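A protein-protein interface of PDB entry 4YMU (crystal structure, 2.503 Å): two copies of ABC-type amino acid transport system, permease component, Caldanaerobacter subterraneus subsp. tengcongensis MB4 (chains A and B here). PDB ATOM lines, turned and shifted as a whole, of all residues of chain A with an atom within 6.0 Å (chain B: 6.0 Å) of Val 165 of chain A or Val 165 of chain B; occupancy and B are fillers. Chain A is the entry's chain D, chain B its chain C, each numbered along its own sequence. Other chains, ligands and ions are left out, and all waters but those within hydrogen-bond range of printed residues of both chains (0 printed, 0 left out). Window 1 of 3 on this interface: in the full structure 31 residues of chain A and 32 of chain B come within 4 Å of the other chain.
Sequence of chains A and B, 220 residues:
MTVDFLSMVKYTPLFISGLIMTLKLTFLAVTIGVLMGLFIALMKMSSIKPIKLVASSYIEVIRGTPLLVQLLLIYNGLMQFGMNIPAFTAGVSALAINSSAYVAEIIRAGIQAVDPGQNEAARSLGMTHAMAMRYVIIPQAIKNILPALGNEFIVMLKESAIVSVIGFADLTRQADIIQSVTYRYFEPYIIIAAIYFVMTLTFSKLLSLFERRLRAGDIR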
ATOM      1  N   LEU A  68       2.089 -17.981 -24.259  1.00  0.00           N
ATOM      2  CA  LEU A  68       1.778 -16.894 -23.327  1.00  0.00           C
ATOM      3  C   LEU A  68       0.642 -16.062 -23.890  1.00  0.00           C
ATOM      4  O   LEU A  68      -0.398 -15.869 -23.227  1.00  0.00           O
ATOM      5  CB  LEU A  68       2.997 -15.989 -23.118  1.00  0.00           C
ATOM      6  CG  LEU A  68       3.285 -15.348 -21.751  1.00  0.00           C
ATOM      7  CD1 LEU A  68       3.974 -14.005 -21.922  1.00  0.00           C
ATOM      8  CD2 LEU A  68       2.050 -15.224 -20.863  1.00  0.00           C
ATOM      9  N   LEU A  71      -2.629 -17.737 -23.604  1.00  0.00           N
ATOM     10  CA  LEU A  71      -3.069 -17.732 -22.209  1.00  0.00           C
ATOM     11  C   LEU A  71      -3.751 -16.408 -21.880  1.00  0.00           C
ATOM     12  O   LEU A  71      -4.910 -16.378 -21.462  1.00  0.00           O
ATOM     13  CB  LEU A  71      -1.878 -17.906 -21.265  1.00  0.00           C
ATOM     14  CG  LEU A  71      -2.018 -18.743 -19.982  1.00  0.00           C
ATOM     15  CD1 LEU A  71      -1.409 -18.026 -18.784  1.00  0.00           C
ATOM     16  CD2 LEU A  71      -3.441 -19.179 -19.703  1.00  0.00           C
ATOM     17  N   LEU A  72      -3.010 -15.319 -22.068  1.00  0.00           N
ATOM     18  CA  LEU A  72      -3.500 -13.984 -21.756  1.00  0.00           C
ATOM     19  C   LEU A  72      -4.725 -13.628 -22.600  1.00  0.00           C
ATOM     20  O   LEU A  72      -5.688 -13.040 -22.091  1.00  0.00           O
ATOM     21  CB  LEU A  72      -2.392 -12.958 -21.990  1.00  0.00           C
ATOM     22  CG  LEU A  72      -1.091 -13.248 -21.249  1.00  0.00           C
ATOM     23  CD1 LEU A  72      -0.111 -12.124 -21.462  1.00  0.00           C
ATOM     24  CD2 LEU A  72      -1.342 -13.485 -19.779  1.00  0.00           C
ATOM     25  N   ALA A 161       4.164 -24.261 -16.341  1.00  0.00           N
ATOM     26  CA  ALA A 161       4.675 -23.301 -15.363  1.00  0.00           C
ATOM     27  C   ALA A 161       4.207 -21.881 -15.678  1.00  0.00           C
ATOM     28  O   ALA A 161       4.296 -20.986 -14.837  1.00  0.00           O
ATOM     29  CB  ALA A 161       6.189 -23.342 -15.306  1.00  0.00           C
ATOM     30  N   ILE A 162       3.710 -21.677 -16.891  1.00  0.00           N
ATOM     31  CA  ILE A 162       3.340 -20.348 -17.334  1.00  0.00           C
ATOM     32  C   ILE A 162       1.981 -19.886 -16.787  1.00  0.00           C
ATOM     33  O   ILE A 162       1.641 -18.710 -16.884  1.00  0.00           O
ATOM     34  CB  ILE A 162       3.359 -20.254 -18.856  1.00  0.00           C
ATOM     35  CG1 ILE A 162       3.742 -18.843 -19.279  1.00  0.00           C
ATOM     36  CG2 ILE A 162       2.024 -20.715 -19.474  1.00  0.00           C
ATOM     37  CD1 ILE A 162       3.517 -18.630 -20.728  1.00  0.00           C
ATOM     38  N   VAL A 163       1.212 -20.794 -16.196  1.00  0.00           N
ATOM     39  CA  VAL A 163      -0.051 -20.390 -15.604  1.00  0.00           C
ATOM     40  C   VAL A 163       0.201 -19.789 -14.221  1.00  0.00           C
ATOM     41  O   VAL A 163      -0.737 -19.409 -13.515  1.00  0.00           O
ATOM     42  CB  VAL A 163      -1.033 -21.563 -15.480  1.00  0.00           C
ATOM     43  CG1 VAL A 163      -1.197 -22.236 -16.830  1.00  0.00           C
ATOM     44  CG2 VAL A 163      -0.540 -22.560 -14.427  1.00  0.00           C
ATOM     45  N   SER A 164       1.469 -19.727 -13.826  1.00  0.00           N
ATOM     46  CA  SER A 164       1.813 -19.105 -12.570  1.00  0.00           C
ATOM     47  C   SER A 164       1.572 -17.599 -12.706  1.00  0.00           C
ATOM     48  O   SER A 164       1.038 -16.970 -11.793  1.00  0.00           O
ATOM     49  CB  SER A 164       3.261 -19.398 -12.181  1.00  0.00           C
ATOM     50  OG  SER A 164       4.155 -18.508 -12.827  1.00  0.00           O
ATOM     51  N   VAL A 165       1.933 -17.028 -13.856  1.00  0.00           N
ATOM     52  CA  VAL A 165       1.810 -15.584 -14.068  1.00  0.00           C
ATOM     53  C   VAL A 165       0.357 -15.093 -14.053  1.00  0.00           C
ATOM     54  O   VAL A 165       0.095 -13.893 -13.963  1.00  0.00           O
ATOM     55  CB  VAL A 165       2.476 -15.126 -15.391  1.00  0.00           C
ATOM     56  CG1 VAL A 165       3.881 -15.708 -15.537  1.00  0.00           C
ATOM     57  CG2 VAL A 165       1.601 -15.487 -16.566  1.00  0.00           C
ATOM     58  N   ILE A 166      -0.576 -16.033 -14.131  1.00  0.00           N
ATOM     59  CA  ILE A 166      -2.008 -15.749 -14.181  1.00  0.00           C
ATOM     60  C   ILE A 166      -2.549 -15.927 -12.771  1.00  0.00           C
ATOM     61  O   ILE A 166      -3.739 -15.796 -12.514  1.00  0.00           O
ATOM     62  CB  ILE A 166      -2.682 -16.753 -15.148  1.00  0.00           C
ATOM     63  CG1 ILE A 166      -3.831 -16.142 -15.929  1.00  0.00           C
ATOM     64  CG2 ILE A 166      -3.200 -18.001 -14.425  1.00  0.00           C
ATOM     65  CD1 ILE A 166      -4.578 -17.222 -16.721  1.00  0.00           C
ATOM     66  N   GLY A 167      -1.651 -16.273 -11.862  1.00  0.00           N
ATOM     67  CA  GLY A 167      -1.998 -16.460 -10.473  1.00  0.00           C
ATOM     68  C   GLY A 167      -2.540 -17.827 -10.118  1.00  0.00           C
ATOM     69  O   GLY A 167      -3.133 -17.995  -9.061  1.00  0.00           O
ATOM     70  N   PHE A 168      -2.338 -18.822 -10.976  1.00  0.00           N
ATOM     71  CA  PHE A 168      -2.759 -20.178 -10.632  1.00  0.00           C
ATOM     72  C   PHE A 168      -1.680 -20.784  -9.743  1.00  0.00           C
ATOM     73  O   PHE A 168      -0.486 -20.530  -9.949  1.00  0.00           O
ATOM     74  CB  PHE A 168      -2.988 -21.022 -11.882  1.00  0.00           C
ATOM     75  CG  PHE A 168      -3.457 -22.421 -11.589  1.00  0.00           C
ATOM     76  CD1 PHE A 168      -4.760 -22.652 -11.160  1.00  0.00           C
ATOM     77  CD2 PHE A 168      -2.594 -23.505 -11.730  1.00  0.00           C
ATOM     78  CE1 PHE A 168      -5.198 -23.939 -10.881  1.00  0.00           C
ATOM     79  CE2 PHE A 168      -3.021 -24.795 -11.449  1.00  0.00           C
ATOM     80  CZ  PHE A 168      -4.325 -25.014 -11.026  1.00  0.00           C
ATOM     81  N   ARG A 173       4.316 -20.938  -8.859  1.00  0.00           N
ATOM     82  CA  ARG A 173       3.667 -19.887  -8.080  1.00  0.00           C
ATOM     83  C   ARG A 173       4.110 -19.914  -6.620  1.00  0.00           C
ATOM     84  O   ARG A 173       4.179 -18.868  -5.977  1.00  0.00           O
ATOM     85  CB  ARG A 173       2.150 -20.015  -8.185  1.00  0.00           C
ATOM     86  CG  ARG A 173       1.364 -18.880  -7.555  1.00  0.00           C
ATOM     87  CD  ARG A 173       1.914 -17.505  -7.931  1.00  0.00           C
ATOM     88  NE  ARG A 173       0.834 -16.528  -8.068  1.00  0.00           N
ATOM     89  CZ  ARG A 173       0.123 -16.028  -7.057  1.00  0.00           C
ATOM     90  NH1 ARG A 173       0.363 -16.403  -5.805  1.00  0.00           N
ATOM     91  NH2 ARG A 173      -0.843 -15.148  -7.299  1.00  0.00           N
ATOM     92  N   LEU B  68      10.917 -20.132 -17.647  1.00  0.00           N
ATOM     93  CA  LEU B  68      10.304 -19.184 -16.717  1.00  0.00           C
ATOM     94  C   LEU B  68      11.036 -19.200 -15.385  1.00  0.00           C
ATOM     95  O   LEU B  68      11.465 -18.148 -14.881  1.00  0.00           O
ATOM     96  CB  LEU B  68       8.846 -19.567 -16.473  1.00  0.00           C
ATOM     97  CG  LEU B  68       7.811 -18.458 -16.230  1.00  0.00           C
ATOM     98  CD1 LEU B  68       6.755 -18.871 -15.188  1.00  0.00           C
ATOM     99  CD2 LEU B  68       8.457 -17.133 -15.869  1.00  0.00           C
ATOM    100  N   LEU B  71      14.360 -17.568 -15.577  1.00  0.00           N
ATOM    101  CA  LEU B  71      14.173 -16.120 -15.630  1.00  0.00           C
ATOM    102  C   LEU B  71      13.996 -15.582 -14.213  1.00  0.00           C
ATOM    103  O   LEU B  71      14.784 -14.764 -13.752  1.00  0.00           O
ATOM    104  CB  LEU B  71      12.907 -15.787 -16.430  1.00  0.00           C
ATOM    105  CG  LEU B  71      12.900 -14.572 -17.366  1.00  0.00           C
ATOM    106  CD1 LEU B  71      11.553 -13.867 -17.323  1.00  0.00           C
ATOM    107  CD2 LEU B  71      14.036 -13.617 -17.069  1.00  0.00           C
ATOM    108  N   LEU B  72      12.972 -16.083 -13.527  1.00  0.00           N
ATOM    109  CA  LEU B  72      12.634 -15.641 -12.180  1.00  0.00           C
ATOM    110  C   LEU B  72      13.776 -15.903 -11.212  1.00  0.00           C
ATOM    111  O   LEU B  72      14.033 -15.090 -10.331  1.00  0.00           O
ATOM    112  CB  LEU B  72      11.350 -16.315 -11.693  1.00  0.00           C
ATOM    113  CG  LEU B  72      10.154 -16.111 -12.625  1.00  0.00           C
ATOM    114  CD1 LEU B  72       8.892 -16.717 -12.047  1.00  0.00           C
ATOM    115  CD2 LEU B  72       9.947 -14.645 -12.943  1.00  0.00           C
ATOM    116  N   ALA B 161       8.559 -13.828 -25.554  1.00  0.00           N
ATOM    117  CA  ALA B 161       7.352 -13.199 -25.056  1.00  0.00           C
ATOM    118  C   ALA B 161       7.291 -13.314 -23.545  1.00  0.00           C
ATOM    119  O   ALA B 161       6.574 -12.563 -22.890  1.00  0.00           O
ATOM    120  CB  ALA B 161       6.125 -13.851 -25.657  1.00  0.00           C
ATOM    121  N   ILE B 162       8.083 -14.216 -22.983  1.00  0.00           N
ATOM    122  CA  ILE B 162       7.987 -14.504 -21.565  1.00  0.00           C
ATOM    123  C   ILE B 162       8.662 -13.464 -20.683  1.00  0.00           C
ATOM    124  O   ILE B 162       8.473 -13.480 -19.477  1.00  0.00           O
ATOM    125  CB  ILE B 162       8.604 -15.864 -21.243  1.00  0.00           C
ATOM    126  CG1 ILE B 162       7.881 -16.499 -20.062  1.00  0.00           C
ATOM    127  CG2 ILE B 162      10.114 -15.738 -20.989  1.00  0.00           C
ATOM    128  CD1 ILE B 162       8.604 -17.696 -19.558  1.00  0.00           C
ATOM    129  N   VAL B 163       9.450 -12.567 -21.267  1.00  0.00           N
ATOM    130  CA  VAL B 163      10.093 -11.524 -20.475  1.00  0.00           C
ATOM    131  C   VAL B 163       9.094 -10.382 -20.258  1.00  0.00           C
ATOM    132  O   VAL B 163       9.383  -9.381 -19.597  1.00  0.00           O
ATOM    133  CB  VAL B 163      11.324 -10.976 -21.180  1.00  0.00           C
ATOM    134  CG1 VAL B 163      12.216 -12.125 -21.616  1.00  0.00           C
ATOM    135  CG2 VAL B 163      10.897 -10.176 -22.396  1.00  0.00           C
ATOM    136  N   SER B 164       7.905 -10.546 -20.815  1.00  0.00           N
ATOM    137  CA  SER B 164       6.880  -9.563 -20.639  1.00  0.00           C
ATOM    138  C   SER B 164       6.468  -9.613 -19.175  1.00  0.00           C
ATOM    139  O   SER B 164       6.304  -8.574 -18.537  1.00  0.00           O
ATOM    140  CB  SER B 164       5.700  -9.884 -21.529  1.00  0.00           C
ATOM    141  OG  SER B 164       4.896 -10.861 -20.904  1.00  0.00           O
ATOM    142  N   VAL B 165       6.370 -10.823 -18.629  1.00  0.00           N
ATOM    143  CA  VAL B 165       5.906 -11.005 -17.258  1.00  0.00           C
ATOM    144  C   VAL B 165       6.859 -10.370 -16.245  1.00  0.00           C
ATOM    145  O   VAL B 165       6.521 -10.196 -15.075  1.00  0.00           O
ATOM    146  CB  VAL B 165       5.770 -12.496 -16.900  1.00  0.00           C
ATOM    147  CG1 VAL B 165       5.112 -13.240 -18.031  1.00  0.00           C
ATOM    148  CG2 VAL B 165       7.136 -13.092 -16.590  1.00  0.00           C
ATOM    149  N   ILE B 166       8.049 -10.026 -16.702  1.00  0.00           N
ATOM    150  CA  ILE B 166       9.079  -9.468 -15.841  1.00  0.00           C
ATOM    151  C   ILE B 166       9.068  -7.951 -16.013  1.00  0.00           C
ATOM    152  O   ILE B 166       9.913  -7.233 -15.468  1.00  0.00           O
ATOM    153  CB  ILE B 166      10.447 -10.100 -16.204  1.00  0.00           C
ATOM    154  CG1 ILE B 166      11.278 -10.397 -14.976  1.00  0.00           C
ATOM    155  CG2 ILE B 166      11.249  -9.269 -17.219  1.00  0.00           C
ATOM    156  CD1 ILE B 166      12.642 -10.834 -15.380  1.00  0.00           C
ATOM    157  N   GLY B 167       8.131  -7.479 -16.833  1.00  0.00           N
ATOM    158  CA  GLY B 167       7.972  -6.058 -17.075  1.00  0.00           C
ATOM    159  C   GLY B 167       8.869  -5.477 -18.152  1.00  0.00           C
ATOM    160  O   GLY B 167       9.046  -4.268 -18.218  1.00  0.00           O
ATOM    161  N   PHE B 168       9.431  -6.325 -19.007  1.00  0.00           N
ATOM    162  CA  PHE B 168      10.225  -5.839 -20.130  1.00  0.00           C
ATOM    163  C   PHE B 168       9.294  -5.424 -21.254  1.00  0.00           C
ATOM    164  O   PHE B 168       8.277  -6.080 -21.498  1.00  0.00           O
ATOM    165  CB  PHE B 168      11.183  -6.916 -20.630  1.00  0.00           C
ATOM    166  CG  PHE B 168      12.020  -6.481 -21.797  1.00  0.00           C
ATOM    167  CD1 PHE B 168      13.057  -5.581 -21.622  1.00  0.00           C
ATOM    168  CD2 PHE B 168      11.763  -6.956 -23.072  1.00  0.00           C
ATOM    169  CE1 PHE B 168      13.814  -5.164 -22.687  1.00  0.00           C
ATOM    170  CE2 PHE B 168      12.532  -6.547 -24.138  1.00  0.00           C
ATOM    171  CZ  PHE B 168      13.560  -5.654 -23.941  1.00  0.00           C
ATOM    172  N   ASP B 170       8.580  -5.767 -24.284  1.00  0.00           N
ATOM    173  CA  ASP B 170       8.626  -6.563 -25.508  1.00  0.00           C
ATOM    174  C   ASP B 170       7.333  -6.389 -26.296  1.00  0.00           C
ATOM    175  O   ASP B 170       6.568  -5.471 -26.041  1.00  0.00           O
ATOM    176  CB  ASP B 170       8.873  -8.038 -25.187  1.00  0.00           C
ATOM    177  CG  ASP B 170       7.644  -8.726 -24.625  1.00  0.00           C
ATOM    178  OD1 ASP B 170       6.877  -8.065 -23.893  1.00  0.00           O
ATOM    179  OD2 ASP B 170       7.437  -9.926 -24.911  1.00  0.00           O
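Hydrophobic or aromatic side chains of chain A that line the printed part of chain B: Leu 68 and Val 165. Hydrophobic or aromatic side chains of chain B within 4 Å of the printed part of chain A: Leu 68 and Val 165.
Of the printed residues of chain B, Val 165 of chain A touches Val 165 (3.7 Å). Of chain A, only Val 165 (3.7 Å) comes within 4 Å of Val 165 of chain B. Of the printed residues of chain A, Ser 164 of chain B touches Leu 68. Printed residues of chain B within 4 Å of Ala 161 of chain A: Leu 68 (3.3 Å). Of the printed residues of chain A, Leu 68 of chain B touches Ala 161 (3.3 Å) and Ser 164 (3.5 Å). Of the printed residues of chain B, Leu 68 of chain A touches Ala 161 and Ser 164. Of the printed residues of chain A, Ala 161 of chain B touches Leu 68 (3.1 Å). Gly 167 of chain A touches none of the printed residues of chain B. Leu 71 of chain A touches none of the printed residues of chain B. The nearest residue of chain A that does not touch Val 165 of chain B is Leu 68 of chain A (4.1 Å).
Among the printed residues, merely in contact across the chains: Leu 68 of chain A with Ala 161 of chain B, Ala 161 of chain A with Leu 68 of chain B, Leu 68 of chain A with Ser 164 of chain B, Ser 164 of chain A with Leu 68 of chain B and Val 165 of chain A with Val 165 of chain B.
The backbone carbonyl oxygen of Ala 161 of chain A sits at hydrogen-bond distance from the side-chain hydroxyl of Ser 164 of chain A (3.2 Å). O of Ala 161 of chain B is in hydrogen-bond range of OG of Ser 164 of chain B, at 3.1 Å.
Leu 68 of chain A touches Ala 161 of chain B, and with the chains exchanged Ala 161 of chain A touches Leu 68 of chain B. Leu 68 of chain A touches Ser 164 of chain B, and with the chains exchanged Ser 164 of chain A touches Leu 68 of chain B. Val 165 of chain B touches its own counterpart, Val 165 of chain A. Positions printed for both chains: 68, 71, 72, 161, 162, 163, 164, 165, 166, 167 and 168. Of the 5 pairs that touch across the chains among the printed residues, 5 have their exchanged pair printed and touching as well.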
